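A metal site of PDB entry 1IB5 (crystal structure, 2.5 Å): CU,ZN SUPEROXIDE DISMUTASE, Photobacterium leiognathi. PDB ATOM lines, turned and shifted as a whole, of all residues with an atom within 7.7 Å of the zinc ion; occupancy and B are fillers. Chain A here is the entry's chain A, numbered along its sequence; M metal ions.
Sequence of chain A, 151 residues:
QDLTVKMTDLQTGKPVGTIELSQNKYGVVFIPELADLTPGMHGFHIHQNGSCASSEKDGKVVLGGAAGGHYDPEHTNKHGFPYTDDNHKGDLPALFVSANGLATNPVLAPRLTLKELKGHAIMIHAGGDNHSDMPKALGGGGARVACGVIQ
The zinc ion is bound by the side-chain carboxylate (OD1) of Asp 91, at 1.9 Å.
ND1 of His 70 is bound to the zinc ion, at 2.1 Å.
The zinc ion is bound by ND1 of His 79 (2.2 Å).
The zinc ion is bound by ND1 of His 88.
The zinc ion has four donor atoms within binding distance.
N of Gly 80 is in hydrogen-bond range of OD2 of Asp 91, 3.0 Å away.
The side-chain amide nitrogen (ND2) of Asn 87 lies within hydrogen-bond range of the side-chain carboxylate (OD2) of Asp 91 (2.9 Å).
NE2 of His 70 lies close to ND1 of His 45 (3.0 Å).
OD1 of Asp 129 sits at hydrogen-bond distance from NE2 of His 79, at 2.8 Å.
N of His 79 sits at hydrogen-bond distance from OD2 of Asp 133 (3.0 Å).
The backbone NH (N) of His 88 is in hydrogen-bond range of the backbone carbonyl oxygen (O) of Lys 78 (2.9 Å).
The backbone carbonyl oxygen (O) of His 88 is in hydrogen-bond range of the guanidinium group (NH2) of Arg 111 (2.7 Å).
The side-chain hydroxyl of Thr 76 sits at hydrogen-bond distance from the backbone NH of His 88 (3.2 Å).
Of the 26 residues printed, 4 come within 4 Å of the zinc ion.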
ATOM      1  N   PHE A  44       9.054   9.188   6.595  1.00  0.00           N
ATOM      2  CA  PHE A  44      10.318   9.039   5.891  1.00  0.00           C
ATOM      3  C   PHE A  44      11.043  10.371   5.870  1.00  0.00           C
ATOM      4  O   PHE A  44      10.593  11.319   5.231  1.00  0.00           O
ATOM      5  CB  PHE A  44       9.986   8.557   4.483  1.00  0.00           C
ATOM      6  CG  PHE A  44      11.155   8.067   3.702  1.00  0.00           C
ATOM      7  CD1 PHE A  44      12.166   7.315   4.301  1.00  0.00           C
ATOM      8  CD2 PHE A  44      11.225   8.316   2.346  1.00  0.00           C
ATOM      9  CE1 PHE A  44      13.187   6.769   3.544  1.00  0.00           C
ATOM     10  CE2 PHE A  44      12.240   7.777   1.594  1.00  0.00           C
ATOM     11  CZ  PHE A  44      13.233   7.023   2.194  1.00  0.00           C
ATOM     12  N   HIS A  45      12.160  10.456   6.582  1.00  0.00           N
ATOM     13  CA  HIS A  45      12.876  11.730   6.652  1.00  0.00           C
ATOM     14  C   HIS A  45      14.391  11.649   6.617  1.00  0.00           C
ATOM     15  O   HIS A  45      14.991  10.604   6.910  1.00  0.00           O
ATOM     16  CB  HIS A  45      12.514  12.447   7.951  1.00  0.00           C
ATOM     17  CG  HIS A  45      11.056  12.402   8.291  1.00  0.00           C
ATOM     18  ND1 HIS A  45      10.606  12.001   9.521  1.00  0.00           N
ATOM     19  CD2 HIS A  45       9.966  12.721   7.562  1.00  0.00           C
ATOM     20  CE1 HIS A  45       9.285  12.065   9.542  1.00  0.00           C
ATOM     21  NE2 HIS A  45       8.875  12.501   8.361  1.00  0.00           N
ATOM     22  N   ILE A  46      15.021  12.758   6.258  1.00  0.00           N
ATOM     23  CA  ILE A  46      16.474  12.833   6.295  1.00  0.00           C
ATOM     24  C   ILE A  46      16.729  13.548   7.623  1.00  0.00           C
ATOM     25  O   ILE A  46      16.097  14.549   7.930  1.00  0.00           O
ATOM     26  CB  ILE A  46      17.046  13.687   5.158  1.00  0.00           C
ATOM     27  CG1 ILE A  46      16.888  12.978   3.802  1.00  0.00           C
ATOM     28  CG2 ILE A  46      18.507  13.972   5.449  1.00  0.00           C
ATOM     29  CD1 ILE A  46      17.615  11.641   3.702  1.00  0.00           C
ATOM     30  N   HIS A  47      17.644  13.013   8.430  1.00  0.00           N
ATOM     31  CA  HIS A  47      17.936  13.640   9.712  1.00  0.00           C
ATOM     32  C   HIS A  47      19.251  14.388   9.743  1.00  0.00           C
ATOM     33  O   HIS A  47      20.087  14.230   8.846  1.00  0.00           O
ATOM     34  CB  HIS A  47      17.871  12.618  10.843  1.00  0.00           C
ATOM     35  CG  HIS A  47      16.470  12.283  11.274  1.00  0.00           C
ATOM     36  ND1 HIS A  47      16.030  12.454  12.560  1.00  0.00           N
ATOM     37  CD2 HIS A  47      15.409  11.828  10.560  1.00  0.00           C
ATOM     38  CE1 HIS A  47      14.754  12.118  12.629  1.00  0.00           C
ATOM     39  NE2 HIS A  47      14.347  11.741  11.437  1.00  0.00           N
ATOM     40  N   GLY A  69      17.425  15.721  15.069  1.00  0.00           N
ATOM     41  CA  GLY A  69      16.150  16.058  14.476  1.00  0.00           C
ATOM     42  C   GLY A  69      16.187  16.024  12.959  1.00  0.00           C
ATOM     43  O   GLY A  69      17.126  15.490  12.360  1.00  0.00           O
ATOM     44  N   HIS A  70      15.170  16.589  12.323  1.00  0.00           N
ATOM     45  CA  HIS A  70      15.101  16.605  10.875  1.00  0.00           C
ATOM     46  C   HIS A  70      16.078  17.596  10.259  1.00  0.00           C
ATOM     47  O   HIS A  70      16.443  18.612  10.866  1.00  0.00           O
ATOM     48  CB  HIS A  70      13.680  16.924  10.415  1.00  0.00           C
ATOM     49  CG  HIS A  70      12.682  15.857  10.772  1.00  0.00           C
ATOM     50  ND1 HIS A  70      11.325  16.015  10.564  1.00  0.00           N
ATOM     51  CD2 HIS A  70      12.851  14.628  11.296  1.00  0.00           C
ATOM     52  CE1 HIS A  70      10.703  14.907  10.956  1.00  0.00           C
ATOM     53  NE2 HIS A  70      11.605  14.054  11.408  1.00  0.00           N
ATOM     54  N   TYR A  71      16.520  17.290   9.053  1.00  0.00           N
ATOM     55  CA  TYR A  71      17.446  18.130   8.329  1.00  0.00           C
ATOM     56  C   TYR A  71      16.719  19.465   8.118  1.00  0.00           C
ATOM     57  O   TYR A  71      15.661  19.510   7.485  1.00  0.00           O
ATOM     58  CB  TYR A  71      17.789  17.446   7.002  1.00  0.00           C
ATOM     59  CG  TYR A  71      18.791  18.160   6.139  1.00  0.00           C
ATOM     60  CD1 TYR A  71      19.994  18.633   6.671  1.00  0.00           C
ATOM     61  CD2 TYR A  71      18.538  18.374   4.779  1.00  0.00           C
ATOM     62  CE1 TYR A  71      20.915  19.294   5.880  1.00  0.00           C
ATOM     63  CE2 TYR A  71      19.462  19.049   3.972  1.00  0.00           C
ATOM     64  CZ  TYR A  71      20.638  19.511   4.525  1.00  0.00           C
ATOM     65  OH  TYR A  71      21.545  20.199   3.744  1.00  0.00           O
ATOM     66  N   ASP A  72      17.282  20.544   8.673  1.00  0.00           N
ATOM     67  CA  ASP A  72      16.679  21.867   8.543  1.00  0.00           C
ATOM     68  C   ASP A  72      17.746  22.923   8.300  1.00  0.00           C
ATOM     69  O   ASP A  72      18.046  23.740   9.166  1.00  0.00           O
ATOM     70  CB  ASP A  72      15.911  22.215   9.829  1.00  0.00           C
ATOM     71  CG  ASP A  72      14.862  23.292   9.612  1.00  0.00           C
ATOM     72  OD1 ASP A  72      14.713  23.771   8.473  1.00  0.00           O
ATOM     73  OD2 ASP A  72      14.199  23.681  10.587  1.00  0.00           O
ATOM     74  N   THR A  76      14.047  26.402   9.836  1.00  0.00           N
ATOM     75  CA  THR A  76      12.642  26.776   9.772  1.00  0.00           C
ATOM     76  C   THR A  76      11.887  26.362  11.033  1.00  0.00           C
ATOM     77  O   THR A  76      10.847  26.930  11.349  1.00  0.00           O
ATOM     78  CB  THR A  76      11.952  26.118   8.572  1.00  0.00           C
ATOM     79  OG1 THR A  76      12.109  24.691   8.663  1.00  0.00           O
ATOM     80  CG2 THR A  76      12.565  26.619   7.275  1.00  0.00           C
ATOM     81  N   LYS A  78      10.011  23.873  11.637  1.00  0.00           N
ATOM     82  CA  LYS A  78       8.658  23.403  11.358  1.00  0.00           C
ATOM     83  C   LYS A  78       8.721  22.135  10.482  1.00  0.00           C
ATOM     84  O   LYS A  78       9.640  21.982   9.673  1.00  0.00           O
ATOM     85  CB  LYS A  78       7.856  24.474  10.604  1.00  0.00           C
ATOM     86  CG  LYS A  78       7.798  25.869  11.239  1.00  0.00           C
ATOM     87  CD  LYS A  78       6.962  26.828  10.371  1.00  0.00           C
ATOM     88  CE  LYS A  78       6.819  28.225  10.972  1.00  0.00           C
ATOM     89  NZ  LYS A  78       8.146  28.877  11.225  1.00  0.00           N
ATOM     90  N   HIS A  79       7.750  21.242  10.653  1.00  0.00           N
ATOM     91  CA  HIS A  79       7.686  20.022   9.864  1.00  0.00           C
ATOM     92  C   HIS A  79       6.582  20.273   8.830  1.00  0.00           C
ATOM     93  O   HIS A  79       5.590  20.919   9.149  1.00  0.00           O
ATOM     94  CB  HIS A  79       7.347  18.812  10.736  1.00  0.00           C
ATOM     95  CG  HIS A  79       7.168  17.541   9.968  1.00  0.00           C
ATOM     96  ND1 HIS A  79       8.218  16.893   9.330  1.00  0.00           N
ATOM     97  CD2 HIS A  79       6.053  16.811   9.680  1.00  0.00           C
ATOM     98  CE1 HIS A  79       7.742  15.826   8.702  1.00  0.00           C
ATOM     99  NE2 HIS A  79       6.452  15.753   8.895  1.00  0.00           N
ATOM    100  N   GLY A  80       6.759  19.795   7.602  1.00  0.00           N
ATOM    101  CA  GLY A  80       5.741  20.015   6.578  1.00  0.00           C
ATOM    102  C   GLY A  80       5.810  19.095   5.373  1.00  0.00           C
ATOM    103  O   GLY A  80       6.155  17.929   5.474  1.00  0.00           O
ATOM    104  N   PHE A  81       5.464  19.632   4.206  1.00  0.00           N
ATOM    105  CA  PHE A  81       5.449  18.837   2.976  1.00  0.00           C
ATOM    106  C   PHE A  81       6.792  18.863   2.227  1.00  0.00           C
ATOM    107  O   PHE A  81       7.677  19.662   2.539  1.00  0.00           O
ATOM    108  CB  PHE A  81       4.363  19.369   2.063  1.00  0.00           C
ATOM    109  CG  PHE A  81       2.966  19.206   2.613  1.00  0.00           C
ATOM    110  CD1 PHE A  81       2.217  18.061   2.335  1.00  0.00           C
ATOM    111  CD2 PHE A  81       2.402  20.199   3.411  1.00  0.00           C
ATOM    112  CE1 PHE A  81       0.917  17.925   2.828  1.00  0.00           C
ATOM    113  CE2 PHE A  81       1.108  20.064   3.913  1.00  0.00           C
ATOM    114  CZ  PHE A  81       0.370  18.920   3.625  1.00  0.00           C
ATOM    115  N   ASN A  87       9.739  24.786   5.725  1.00  0.00           N
ATOM    116  CA  ASN A  87       9.847  23.687   6.674  1.00  0.00           C
ATOM    117  C   ASN A  87      11.071  22.837   6.370  1.00  0.00           C
ATOM    118  O   ASN A  87      11.732  23.004   5.345  1.00  0.00           O
ATOM    119  CB  ASN A  87       8.590  22.797   6.702  1.00  0.00           C
ATOM    120  CG  ASN A  87       8.132  22.355   5.326  1.00  0.00           C
ATOM    121  OD1 ASN A  87       7.386  23.056   4.660  1.00  0.00           O
ATOM    122  ND2 ASN A  87       8.596  21.180   4.891  1.00  0.00           N
ATOM    123  N   HIS A  88      11.383  21.944   7.296  1.00  0.00           N
ATOM    124  CA  HIS A  88      12.510  21.032   7.209  1.00  0.00           C
ATOM    125  C   HIS A  88      12.766  20.621   5.752  1.00  0.00           C
ATOM    126  O   HIS A  88      11.899  20.028   5.129  1.00  0.00           O
ATOM    127  CB  HIS A  88      12.226  19.779   8.041  1.00  0.00           C
ATOM    128  CG  HIS A  88      11.926  20.070   9.470  1.00  0.00           C
ATOM    129  ND1 HIS A  88      11.029  19.334  10.223  1.00  0.00           N
ATOM    130  CD2 HIS A  88      12.407  21.033  10.299  1.00  0.00           C
ATOM    131  CE1 HIS A  88      10.979  19.828  11.450  1.00  0.00           C
ATOM    132  NE2 HIS A  88      11.797  20.859  11.517  1.00  0.00           N
ATOM    133  N   LYS A  89      13.946  20.940   5.232  1.00  0.00           N
ATOM    134  CA  LYS A  89      14.259  20.580   3.852  1.00  0.00           C
ATOM    135  C   LYS A  89      14.331  19.055   3.803  1.00  0.00           C
ATOM    136  O   LYS A  89      14.314  18.453   2.721  1.00  0.00           O
ATOM    137  CB  LYS A  89      15.598  21.178   3.389  1.00  0.00           C
ATOM    138  CG  LYS A  89      15.621  21.520   1.879  1.00  0.00           C
ATOM    139  CD  LYS A  89      17.019  21.847   1.322  1.00  0.00           C
ATOM    140  CE  LYS A  89      17.609  23.109   1.950  1.00  0.00           C
ATOM    141  NZ  LYS A  89      18.980  23.390   1.420  1.00  0.00           N
ATOM    142  N   GLY A  90      14.388  18.422   4.984  1.00  0.00           N
ATOM    143  CA  GLY A  90      14.472  16.964   5.060  1.00  0.00           C
ATOM    144  C   GLY A  90      13.149  16.237   5.123  1.00  0.00           C
ATOM    145  O   GLY A  90      13.110  15.042   5.412  1.00  0.00           O
ATOM    146  N   ASP A  91      12.059  16.944   4.854  1.00  0.00           N
ATOM    147  CA  ASP A  91      10.743  16.346   4.857  1.00  0.00           C
ATOM    148  C   ASP A  91      10.477  15.665   3.509  1.00  0.00           C
ATOM    149  O   ASP A  91      10.222  16.309   2.501  1.00  0.00           O
ATOM    150  CB  ASP A  91       9.710  17.422   5.160  1.00  0.00           C
ATOM    151  CG  ASP A  91       9.887  18.005   6.541  1.00  0.00           C
ATOM    152  OD1 ASP A  91      10.368  17.255   7.416  1.00  0.00           O
ATOM    153  OD2 ASP A  91       9.531  19.179   6.772  1.00  0.00           O
ATOM    154  N   LEU A  92      10.573  14.344   3.520  1.00  0.00           N
ATOM    155  CA  LEU A  92      10.373  13.524   2.328  1.00  0.00           C
ATOM    156  C   LEU A  92       8.931  13.008   2.282  1.00  0.00           C
ATOM    157  O   LEU A  92       8.202  13.109   3.254  1.00  0.00           O
ATOM    158  CB  LEU A  92      11.321  12.325   2.394  1.00  0.00           C
ATOM    159  CG  LEU A  92      12.832  12.552   2.613  1.00  0.00           C
ATOM    160  CD1 LEU A  92      13.558  11.216   2.734  1.00  0.00           C
ATOM    161  CD2 LEU A  92      13.388  13.325   1.434  1.00  0.00           C
ATOM    162  N   ARG A 111      13.004  19.568  -3.274  1.00  0.00           N
ATOM    163  CA  ARG A 111      13.875  20.561  -2.650  1.00  0.00           C
ATOM    164  C   ARG A 111      15.271  20.066  -2.292  1.00  0.00           C
ATOM    165  O   ARG A 111      16.039  20.795  -1.643  1.00  0.00           O
ATOM    166  CB  ARG A 111      13.200  21.114  -1.386  1.00  0.00           C
ATOM    167  CG  ARG A 111      11.866  21.831  -1.612  1.00  0.00           C
ATOM    168  CD  ARG A 111      11.472  22.664  -0.390  1.00  0.00           C
ATOM    169  NE  ARG A 111      11.052  21.853   0.747  1.00  0.00           N
ATOM    170  CZ  ARG A 111      11.373  22.126   2.009  1.00  0.00           C
ATOM    171  NH1 ARG A 111      12.105  23.183   2.298  1.00  0.00           N
ATOM    172  NH2 ARG A 111      10.933  21.339   2.991  1.00  0.00           N
ATOM    173  N   ASP A 129       2.921  10.066   8.567  1.00  0.00           N
ATOM    174  CA  ASP A 129       3.372  11.447   8.491  1.00  0.00           C
ATOM    175  C   ASP A 129       2.271  12.271   7.816  1.00  0.00           C
ATOM    176  O   ASP A 129       1.980  12.052   6.653  1.00  0.00           O
ATOM    177  CB  ASP A 129       4.651  11.499   7.636  1.00  0.00           C
ATOM    178  CG  ASP A 129       5.271  12.887   7.564  1.00  0.00           C
ATOM    179  OD1 ASP A 129       4.648  13.884   7.981  1.00  0.00           O
ATOM    180  OD2 ASP A 129       6.421  12.975   7.082  1.00  0.00           O
ATOM    181  N   HIS A 131       2.515  15.384   7.459  1.00  0.00           N
ATOM    182  CA  HIS A 131       3.267  16.574   7.069  1.00  0.00           C
ATOM    183  C   HIS A 131       2.852  17.864   7.749  1.00  0.00           C
ATOM    184  O   HIS A 131       2.637  18.879   7.080  1.00  0.00           O
ATOM    185  CB  HIS A 131       3.193  16.760   5.553  1.00  0.00           C
ATOM    186  CG  HIS A 131       3.698  15.574   4.787  1.00  0.00           C
ATOM    187  ND1 HIS A 131       2.864  14.616   4.258  1.00  0.00           N
ATOM    188  CD2 HIS A 131       4.965  15.193   4.485  1.00  0.00           C
ATOM    189  CE1 HIS A 131       3.597  13.690   3.651  1.00  0.00           C
ATOM    190  NE2 HIS A 131       4.864  14.026   3.771  1.00  0.00           N
ATOM    191  N   SER A 132       2.774  17.835   9.073  1.00  0.00           N
ATOM    192  CA  SER A 132       2.422  18.991   9.874  1.00  0.00           C
ATOM    193  C   SER A 132       2.871  18.698  11.291  1.00  0.00           C
ATOM    194  O   SER A 132       3.350  17.595  11.586  1.00  0.00           O
ATOM    195  CB  SER A 132       0.903  19.200   9.857  1.00  0.00           C
ATOM    196  OG  SER A 132       0.492  20.122  10.862  1.00  0.00           O
ATOM    197  N   ASP A 133       2.718  19.676  12.182  1.00  0.00           N
ATOM    198  CA  ASP A 133       3.086  19.500  13.587  1.00  0.00           C
ATOM    199  C   ASP A 133       1.830  19.365  14.434  1.00  0.00           C
ATOM    200  O   ASP A 133       1.885  19.424  15.665  1.00  0.00           O
ATOM    201  CB  ASP A 133       3.937  20.674  14.104  1.00  0.00           C
ATOM    202  CG  ASP A 133       5.397  20.596  13.647  1.00  0.00           C
ATOM    203  OD1 ASP A 133       6.096  19.623  13.981  1.00  0.00           O
ATOM    204  OD2 ASP A 133       5.844  21.537  12.952  1.00  0.00           O
ATOM    205  N   LEU A 138       5.968  16.525  14.215  1.00  0.00           N
ATOM    206  CA  LEU A 138       6.721  15.770  13.235  1.00  0.00           C
ATOM    207  C   LEU A 138       5.860  14.806  12.405  1.00  0.00           C
ATOM    208  O   LEU A 138       6.342  13.783  11.937  1.00  0.00           O
ATOM    209  CB  LEU A 138       7.840  15.013  13.953  1.00  0.00           C
ATOM    210  CG  LEU A 138       8.741  15.939  14.781  1.00  0.00           C
ATOM    211  CD1 LEU A 138       9.784  15.137  15.566  1.00  0.00           C
ATOM    212  CD2 LEU A 138       9.427  16.924  13.847  1.00  0.00           C
ATOM    213  N   GLY A 139       4.576  15.139  12.235  1.00  0.00           N
ATOM    214  CA  GLY A 139       3.694  14.301  11.445  1.00  0.00           C
ATOM    215  C   GLY A 139       3.178  13.030  12.105  1.00  0.00           C
ATOM    216  O   GLY A 139       2.454  12.250  11.479  1.00  0.00           O
HETATM  217 ZN    ZN M   1      10.351  17.416   9.342  1.00  0.00          ZN
HETATM  218 CU    CU M   2      12.218  11.551  10.980  1.00  0.00          CU
